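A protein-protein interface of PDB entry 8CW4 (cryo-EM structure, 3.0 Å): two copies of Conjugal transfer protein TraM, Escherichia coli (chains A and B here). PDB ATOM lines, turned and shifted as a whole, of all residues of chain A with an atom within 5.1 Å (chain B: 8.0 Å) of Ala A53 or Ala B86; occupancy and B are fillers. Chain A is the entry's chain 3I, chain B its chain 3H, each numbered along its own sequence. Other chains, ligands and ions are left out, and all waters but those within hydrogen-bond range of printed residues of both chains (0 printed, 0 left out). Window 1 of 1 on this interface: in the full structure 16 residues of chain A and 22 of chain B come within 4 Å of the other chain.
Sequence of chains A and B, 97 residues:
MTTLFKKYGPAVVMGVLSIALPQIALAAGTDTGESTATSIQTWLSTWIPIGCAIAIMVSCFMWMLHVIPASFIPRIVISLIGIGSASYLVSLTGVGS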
ATOM      1  N   PRO A  49       0.107 -24.427  20.593  1.00  0.00           N
ATOM      2  CA  PRO A  49      -0.360 -24.702  19.225  1.00  0.00           C
ATOM      3  C   PRO A  49      -1.694 -25.422  19.162  1.00  0.00           C
ATOM      4  O   PRO A  49      -2.503 -25.122  18.276  1.00  0.00           O
ATOM      5  CB  PRO A  49       0.768 -25.559  18.638  1.00  0.00           C
ATOM      6  CG  PRO A  49       1.968 -25.180  19.407  1.00  0.00           C
ATOM      7  CD  PRO A  49       1.522 -24.780  20.780  1.00  0.00           C
ATOM      8  N   ILE A  50      -1.956 -26.368  20.065  1.00  0.00           N
ATOM      9  CA  ILE A  50      -3.245 -27.055  20.058  1.00  0.00           C
ATOM     10  C   ILE A  50      -4.363 -26.093  20.428  1.00  0.00           C
ATOM     11  O   ILE A  50      -5.465 -26.157  19.873  1.00  0.00           O
ATOM     12  CB  ILE A  50      -3.211 -28.276  20.993  1.00  0.00           C
ATOM     13  CG1 ILE A  50      -1.951 -29.099  20.735  1.00  0.00           C
ATOM     14  CG2 ILE A  50      -4.448 -29.123  20.792  1.00  0.00           C
ATOM     15  CD1 ILE A  50      -1.749 -30.219  21.714  1.00  0.00           C
ATOM     16  N   GLY A  51      -4.106 -25.197  21.380  1.00  0.00           N
ATOM     17  CA  GLY A  51      -5.096 -24.192  21.722  1.00  0.00           C
ATOM     18  C   GLY A  51      -5.409 -23.256  20.573  1.00  0.00           C
ATOM     19  O   GLY A  51      -6.540 -22.779  20.448  1.00  0.00           O
ATOM     20  N   CYS A  52      -4.417 -22.969  19.729  1.00  0.00           N
ATOM     21  CA  CYS A  52      -4.654 -22.118  18.567  1.00  0.00           C
ATOM     22  C   CYS A  52      -5.609 -22.779  17.583  1.00  0.00           C
ATOM     23  O   CYS A  52      -6.456 -22.106  16.988  1.00  0.00           O
ATOM     24  CB  CYS A  52      -3.330 -21.780  17.883  1.00  0.00           C
ATOM     25  SG  CYS A  52      -2.296 -20.622  18.796  1.00  0.00           S
ATOM     26  N   ALA A  53      -5.479 -24.092  17.385  1.00  0.00           N
ATOM     27  CA  ALA A  53      -6.389 -24.794  16.489  1.00  0.00           C
ATOM     28  C   ALA A  53      -7.813 -24.788  17.029  1.00  0.00           C
ATOM     29  O   ALA A  53      -8.773 -24.726  16.255  1.00  0.00           O
ATOM     30  CB  ALA A  53      -5.905 -26.226  16.266  1.00  0.00           C
ATOM     31  N   ILE A  54      -7.969 -24.863  18.351  1.00  0.00           N
ATOM     32  CA  ILE A  54      -9.304 -24.833  18.944  1.00  0.00           C
ATOM     33  C   ILE A  54      -9.984 -23.501  18.660  1.00  0.00           C
ATOM     34  O   ILE A  54     -11.174 -23.453  18.330  1.00  0.00           O
ATOM     35  CB  ILE A  54      -9.226 -25.115  20.456  1.00  0.00           C
ATOM     36  CG1 ILE A  54      -8.863 -26.575  20.708  1.00  0.00           C
ATOM     37  CG2 ILE A  54     -10.544 -24.786  21.125  1.00  0.00           C
ATOM     38  CD1 ILE A  54      -8.511 -26.870  22.142  1.00  0.00           C
ATOM     39  N   ALA A  55      -9.244 -22.398  18.788  1.00  0.00           N
ATOM     40  CA  ALA A  55      -9.832 -21.082  18.560  1.00  0.00           C
ATOM     41  C   ALA A  55     -10.313 -20.928  17.123  1.00  0.00           C
ATOM     42  O   ALA A  55     -11.382 -20.360  16.878  1.00  0.00           O
ATOM     43  CB  ALA A  55      -8.823 -19.989  18.907  1.00  0.00           C
ATOM     44  N   ILE A  56      -9.536 -21.423  16.158  1.00  0.00           N
ATOM     45  CA  ILE A  56      -9.942 -21.328  14.759  1.00  0.00           C
ATOM     46  C   ILE A  56     -11.251 -22.073  14.535  1.00  0.00           C
ATOM     47  O   ILE A  56     -12.158 -21.582  13.853  1.00  0.00           O
ATOM     48  CB  ILE A  56      -8.830 -21.857  13.839  1.00  0.00           C
ATOM     49  CG1 ILE A  56      -7.537 -21.077  14.057  1.00  0.00           C
ATOM     50  CG2 ILE A  56      -9.255 -21.767  12.389  1.00  0.00           C
ATOM     51  CD1 ILE A  56      -6.516 -21.297  12.969  1.00  0.00           C
ATOM     52  N   MET A  57     -11.364 -23.279  15.095  1.00  0.00           N
ATOM     53  CA  MET A  57     -12.586 -24.058  14.935  1.00  0.00           C
ATOM     54  C   MET A  57     -13.771 -23.390  15.618  1.00  0.00           C
ATOM     55  O   MET A  57     -14.871 -23.341  15.056  1.00  0.00           O
ATOM     56  CB  MET A  57     -12.379 -25.469  15.480  1.00  0.00           C
ATOM     57  CG  MET A  57     -13.626 -26.329  15.469  1.00  0.00           C
ATOM     58  SD  MET A  57     -13.315 -28.008  16.037  1.00  0.00           S
ATOM     59  CE  MET A  57     -12.763 -27.702  17.710  1.00  0.00           C
ATOM     60  N   GLN B  41     -10.055 -30.559  22.605  1.00  0.00           N
ATOM     61  CA  GLN B  41     -10.275 -30.580  21.164  1.00  0.00           C
ATOM     62  C   GLN B  41     -11.143 -31.762  20.752  1.00  0.00           C
ATOM     63  O   GLN B  41     -12.036 -31.624  19.910  1.00  0.00           O
ATOM     64  CB  GLN B  41      -8.939 -30.625  20.427  1.00  0.00           C
ATOM     65  CG  GLN B  41      -8.997 -30.082  19.018  1.00  0.00           C
ATOM     66  CD  GLN B  41      -7.677 -30.201  18.298  1.00  0.00           C
ATOM     67  OE1 GLN B  41      -6.833 -31.016  18.661  1.00  0.00           O
ATOM     68  NE2 GLN B  41      -7.488 -29.390  17.268  1.00  0.00           N
ATOM     69  N   LEU B  44     -14.942 -31.195  21.710  1.00  0.00           N
ATOM     70  CA  LEU B  44     -15.690 -30.250  20.889  1.00  0.00           C
ATOM     71  C   LEU B  44     -16.124 -30.883  19.574  1.00  0.00           C
ATOM     72  O   LEU B  44     -17.237 -30.639  19.096  1.00  0.00           O
ATOM     73  CB  LEU B  44     -14.853 -29.000  20.631  1.00  0.00           C
ATOM     74  CG  LEU B  44     -14.651 -28.060  21.818  1.00  0.00           C
ATOM     75  CD1 LEU B  44     -13.704 -26.940  21.446  1.00  0.00           C
ATOM     76  CD2 LEU B  44     -15.974 -27.501  22.294  1.00  0.00           C
ATOM     77  N   LEU B  80     -17.211 -24.028   6.960  1.00  0.00           N
ATOM     78  CA  LEU B  80     -16.930 -25.458   7.000  1.00  0.00           C
ATOM     79  C   LEU B  80     -15.506 -25.755   6.550  1.00  0.00           C
ATOM     80  O   LEU B  80     -14.875 -26.693   7.048  1.00  0.00           O
ATOM     81  CB  LEU B  80     -17.935 -26.218   6.139  1.00  0.00           C
ATOM     82  CG  LEU B  80     -19.378 -26.263   6.638  1.00  0.00           C
ATOM     83  CD1 LEU B  80     -20.265 -26.926   5.605  1.00  0.00           C
ATOM     84  CD2 LEU B  80     -19.462 -26.995   7.959  1.00  0.00           C
ATOM     85  N   ILE B  81     -14.987 -24.982   5.596  1.00  0.00           N
ATOM     86  CA  ILE B  81     -13.597 -25.148   5.178  1.00  0.00           C
ATOM     87  C   ILE B  81     -12.658 -24.842   6.337  1.00  0.00           C
ATOM     88  O   ILE B  81     -11.671 -25.548   6.564  1.00  0.00           O
ATOM     89  CB  ILE B  81     -13.293 -24.264   3.957  1.00  0.00           C
ATOM     90  CG1 ILE B  81     -13.913 -24.862   2.695  1.00  0.00           C
ATOM     91  CG2 ILE B  81     -11.799 -24.099   3.780  1.00  0.00           C
ATOM     92  CD1 ILE B  81     -13.721 -24.014   1.466  1.00  0.00           C
ATOM     93  N   GLY B  82     -12.947 -23.772   7.080  1.00  0.00           N
ATOM     94  CA  GLY B  82     -12.084 -23.399   8.190  1.00  0.00           C
ATOM     95  C   GLY B  82     -12.113 -24.398   9.328  1.00  0.00           C
ATOM     96  O   GLY B  82     -11.083 -24.676   9.946  1.00  0.00           O
ATOM     97  N   ILE B  83     -13.291 -24.943   9.633  1.00  0.00           N
ATOM     98  CA  ILE B  83     -13.404 -25.893  10.735  1.00  0.00           C
ATOM     99  C   ILE B  83     -12.604 -27.156  10.458  1.00  0.00           C
ATOM    100  O   ILE B  83     -11.918 -27.671  11.348  1.00  0.00           O
ATOM    101  CB  ILE B  83     -14.882 -26.220  11.013  1.00  0.00           C
ATOM    102  CG1 ILE B  83     -15.588 -25.017  11.633  1.00  0.00           C
ATOM    103  CG2 ILE B  83     -15.000 -27.428  11.914  1.00  0.00           C
ATOM    104  CD1 ILE B  83     -17.089 -25.092  11.558  1.00  0.00           C
ATOM    105  N   GLY B  84     -12.677 -27.684   9.237  1.00  0.00           N
ATOM    106  CA  GLY B  84     -11.980 -28.919   8.932  1.00  0.00           C
ATOM    107  C   GLY B  84     -10.493 -28.740   8.704  1.00  0.00           C
ATOM    108  O   GLY B  84      -9.736 -29.713   8.753  1.00  0.00           O
ATOM    109  N   SER B  85     -10.054 -27.509   8.450  1.00  0.00           N
ATOM    110  CA  SER B  85      -8.654 -27.216   8.169  1.00  0.00           C
ATOM    111  C   SER B  85      -7.951 -26.512   9.322  1.00  0.00           C
ATOM    112  O   SER B  85      -6.879 -25.939   9.120  1.00  0.00           O
ATOM    113  CB  SER B  85      -8.541 -26.370   6.901  1.00  0.00           C
ATOM    114  OG  SER B  85      -9.074 -27.053   5.784  1.00  0.00           O
ATOM    115  N   ALA B  86      -8.529 -26.535  10.524  1.00  0.00           N
ATOM    116  CA  ALA B  86      -7.958 -25.786  11.637  1.00  0.00           C
ATOM    117  C   ALA B  86      -6.553 -26.269  11.976  1.00  0.00           C
ATOM    118  O   ALA B  86      -5.624 -25.466  12.112  1.00  0.00           O
ATOM    119  CB  ALA B  86      -8.872 -25.892  12.857  1.00  0.00           C
ATOM    120  N   SER B  87      -6.379 -27.583  12.128  1.00  0.00           N
ATOM    121  CA  SER B  87      -5.072 -28.122  12.492  1.00  0.00           C
ATOM    122  C   SER B  87      -4.050 -27.903  11.384  1.00  0.00           C
ATOM    123  O   SER B  87      -2.895 -27.560  11.657  1.00  0.00           O
ATOM    124  CB  SER B  87      -5.188 -29.607  12.823  1.00  0.00           C
ATOM    125  OG  SER B  87      -5.978 -29.810  13.979  1.00  0.00           O
ATOM    126  N   TYR B  88      -4.453 -28.114  10.130  1.00  0.00           N
ATOM    127  CA  TYR B  88      -3.525 -27.943   9.017  1.00  0.00           C
ATOM    128  C   TYR B  88      -3.083 -26.493   8.885  1.00  0.00           C
ATOM    129  O   TYR B  88      -1.912 -26.213   8.607  1.00  0.00           O
ATOM    130  CB  TYR B  88      -4.170 -28.431   7.722  1.00  0.00           C
ATOM    131  CG  TYR B  88      -3.396 -28.085   6.476  1.00  0.00           C
ATOM    132  CD1 TYR B  88      -2.312 -28.848   6.078  1.00  0.00           C
ATOM    133  CD2 TYR B  88      -3.757 -27.001   5.692  1.00  0.00           C
ATOM    134  CE1 TYR B  88      -1.605 -28.538   4.939  1.00  0.00           C
ATOM    135  CE2 TYR B  88      -3.054 -26.682   4.555  1.00  0.00           C
ATOM    136  CZ  TYR B  88      -1.979 -27.455   4.182  1.00  0.00           C
ATOM    137  OH  TYR B  88      -1.276 -27.143   3.045  1.00  0.00           O
ATOM    138  N   LEU B  89      -4.011 -25.555   9.071  1.00  0.00           N
ATOM    139  CA  LEU B  89      -3.682 -24.143   8.906  1.00  0.00           C
ATOM    140  C   LEU B  89      -2.673 -23.678   9.948  1.00  0.00           C
ATOM    141  O   LEU B  89      -1.788 -22.872   9.643  1.00  0.00           O
ATOM    142  CB  LEU B  89      -4.957 -23.303   8.975  1.00  0.00           C
ATOM    143  CG  LEU B  89      -5.850 -23.387   7.739  1.00  0.00           C
ATOM    144  CD1 LEU B  89      -7.130 -22.600   7.942  1.00  0.00           C
ATOM    145  CD2 LEU B  89      -5.106 -22.888   6.518  1.00  0.00           C
ATOM    146  N   VAL B  90      -2.797 -24.161  11.185  1.00  0.00           N
ATOM    147  CA  VAL B  90      -1.886 -23.724  12.240  1.00  0.00           C
ATOM    148  C   VAL B  90      -0.457 -24.142  11.926  1.00  0.00           C
ATOM    149  O   VAL B  90       0.479 -23.344  12.047  1.00  0.00           O
ATOM    150  CB  VAL B  90      -2.345 -24.268  13.604  1.00  0.00           C
ATOM    151  CG1 VAL B  90      -1.287 -24.009  14.655  1.00  0.00           C
ATOM    152  CG2 VAL B  90      -3.659 -23.634  14.004  1.00  0.00           C
ATOM    153  N   SER B  91      -0.261 -25.398  11.518  1.00  0.00           N
ATOM    154  CA  SER B  91       1.088 -25.871  11.227  1.00  0.00           C
ATOM    155  C   SER B  91       1.614 -25.295   9.921  1.00  0.00           C
ATOM    156  O   SER B  91       2.831 -25.244   9.713  1.00  0.00           O
ATOM    157  CB  SER B  91       1.115 -27.395  11.174  1.00  0.00           C
ATOM    158  OG  SER B  91       0.354 -27.878  10.082  1.00  0.00           O
ATOM    159  N   LEU B  92       0.721 -24.863   9.033  1.00  0.00           N
ATOM    160  CA  LEU B  92       1.154 -24.253   7.782  1.00  0.00           C
ATOM    161  C   LEU B  92       1.958 -22.984   8.026  1.00  0.00           C
ATOM    162  O   LEU B  92       2.793 -22.610   7.196  1.00  0.00           O
ATOM    163  CB  LEU B  92      -0.060 -23.958   6.905  1.00  0.00           C
ATOM    164  CG  LEU B  92       0.168 -23.368   5.518  1.00  0.00           C
ATOM    165  CD1 LEU B  92       0.554 -24.449   4.529  1.00  0.00           C
ATOM    166  CD2 LEU B  92      -1.084 -22.646   5.061  1.00  0.00           C
ATOM    167  N   VAL B  95       3.830 -22.757  13.388  1.00  0.00           N
ATOM    168  CA  VAL B  95       3.587 -22.838  14.822  1.00  0.00           C
ATOM    169  C   VAL B  95       3.378 -24.291  15.224  1.00  0.00           C
ATOM    170  O   VAL B  95       2.672 -25.051  14.553  1.00  0.00           O
ATOM    171  CB  VAL B  95       2.380 -21.965  15.219  1.00  0.00           C
ATOM    172  CG1 VAL B  95       2.034 -22.173  16.679  1.00  0.00           C
ATOM    173  CG2 VAL B  95       2.672 -20.507  14.950  1.00  0.00           C
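Pro A49 touches Val B90 (O to CG1, 3.98 Å).
Gln B41 touches Ile A50 (OE1 to CG2, 3.7 Å).
Gln B41 touches Ala A53 (NE2 to CB, 3.7 Å).
Ala A53 touches Ala B86.
Ala A53 touches Val B90.
CG of Gln B41 touches CG1 of Ile A54, at 3.9 Å.
Ile A54 touches Leu B44.
Ile A56 touches Val B90.
CB of Leu B44 touches CE of Met A57, at 3.8 Å.
Met A57 touches Ile B83 (O to CG1, 3.9 Å).
Printed residues of chain B within 4 Å of Ala A53: Gln B41 (3.7 Å), Ala B86 (3.6 Å) and Val B90 (3.9 Å).
Printed residues of chain B within 4 Å of Ile A56: Val B90 (3.8 Å).
Printed residues of chain B within 4 Å of Met A57: Leu B44 and Ile B83.
Of the printed residues of chain A, Leu B44 touches Ile A54 (3.8 Å) and Met A57 (3.8 Å).
Printed residues of chain A within 4 Å of Ile B83: Met A57.
Ala B86 touches one residue of chain A.
Of the printed residues of chain A, Val B90 touches Pro A49, Ala A53 and Ile A56.
Ser B91 touches none of the printed residues of chain A.
The nearest residue of chain B that does not touch Ala A53 is Ser B87 (4.3 Å).
The nearest residue of chain A that does not touch Ala B86 is Ile A56 (4.2 Å).
The nearest printed residue of chain A that does not touch Val B90 is Cys A52 (4.2 Å).
Of the 9 printed residues of chain A, 6 touch a printed residue of chain B.
Printed residues of chain A that touch a printed residue of chain B: Pro A49, Ile A50, Ala A53, Ile A54, Ile A56 and Met A57.
Hydrophobic or aromatic side chains of chain A that line the printed part of chain B: Ile A50, Ala A53, Ile A54, Ile A56 and Met A57.
Among the printed residues, 10 pairs touch across the chains.
Among the printed residues, no Asp or Glu carboxylate lies within 4 Å of a Lys or Arg side-chain nitrogen of the other chain.
No position is printed for both chains.
Of the 10 pairs that touch across the chains among the printed residues, none has its exchanged pair printed and touching as well.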
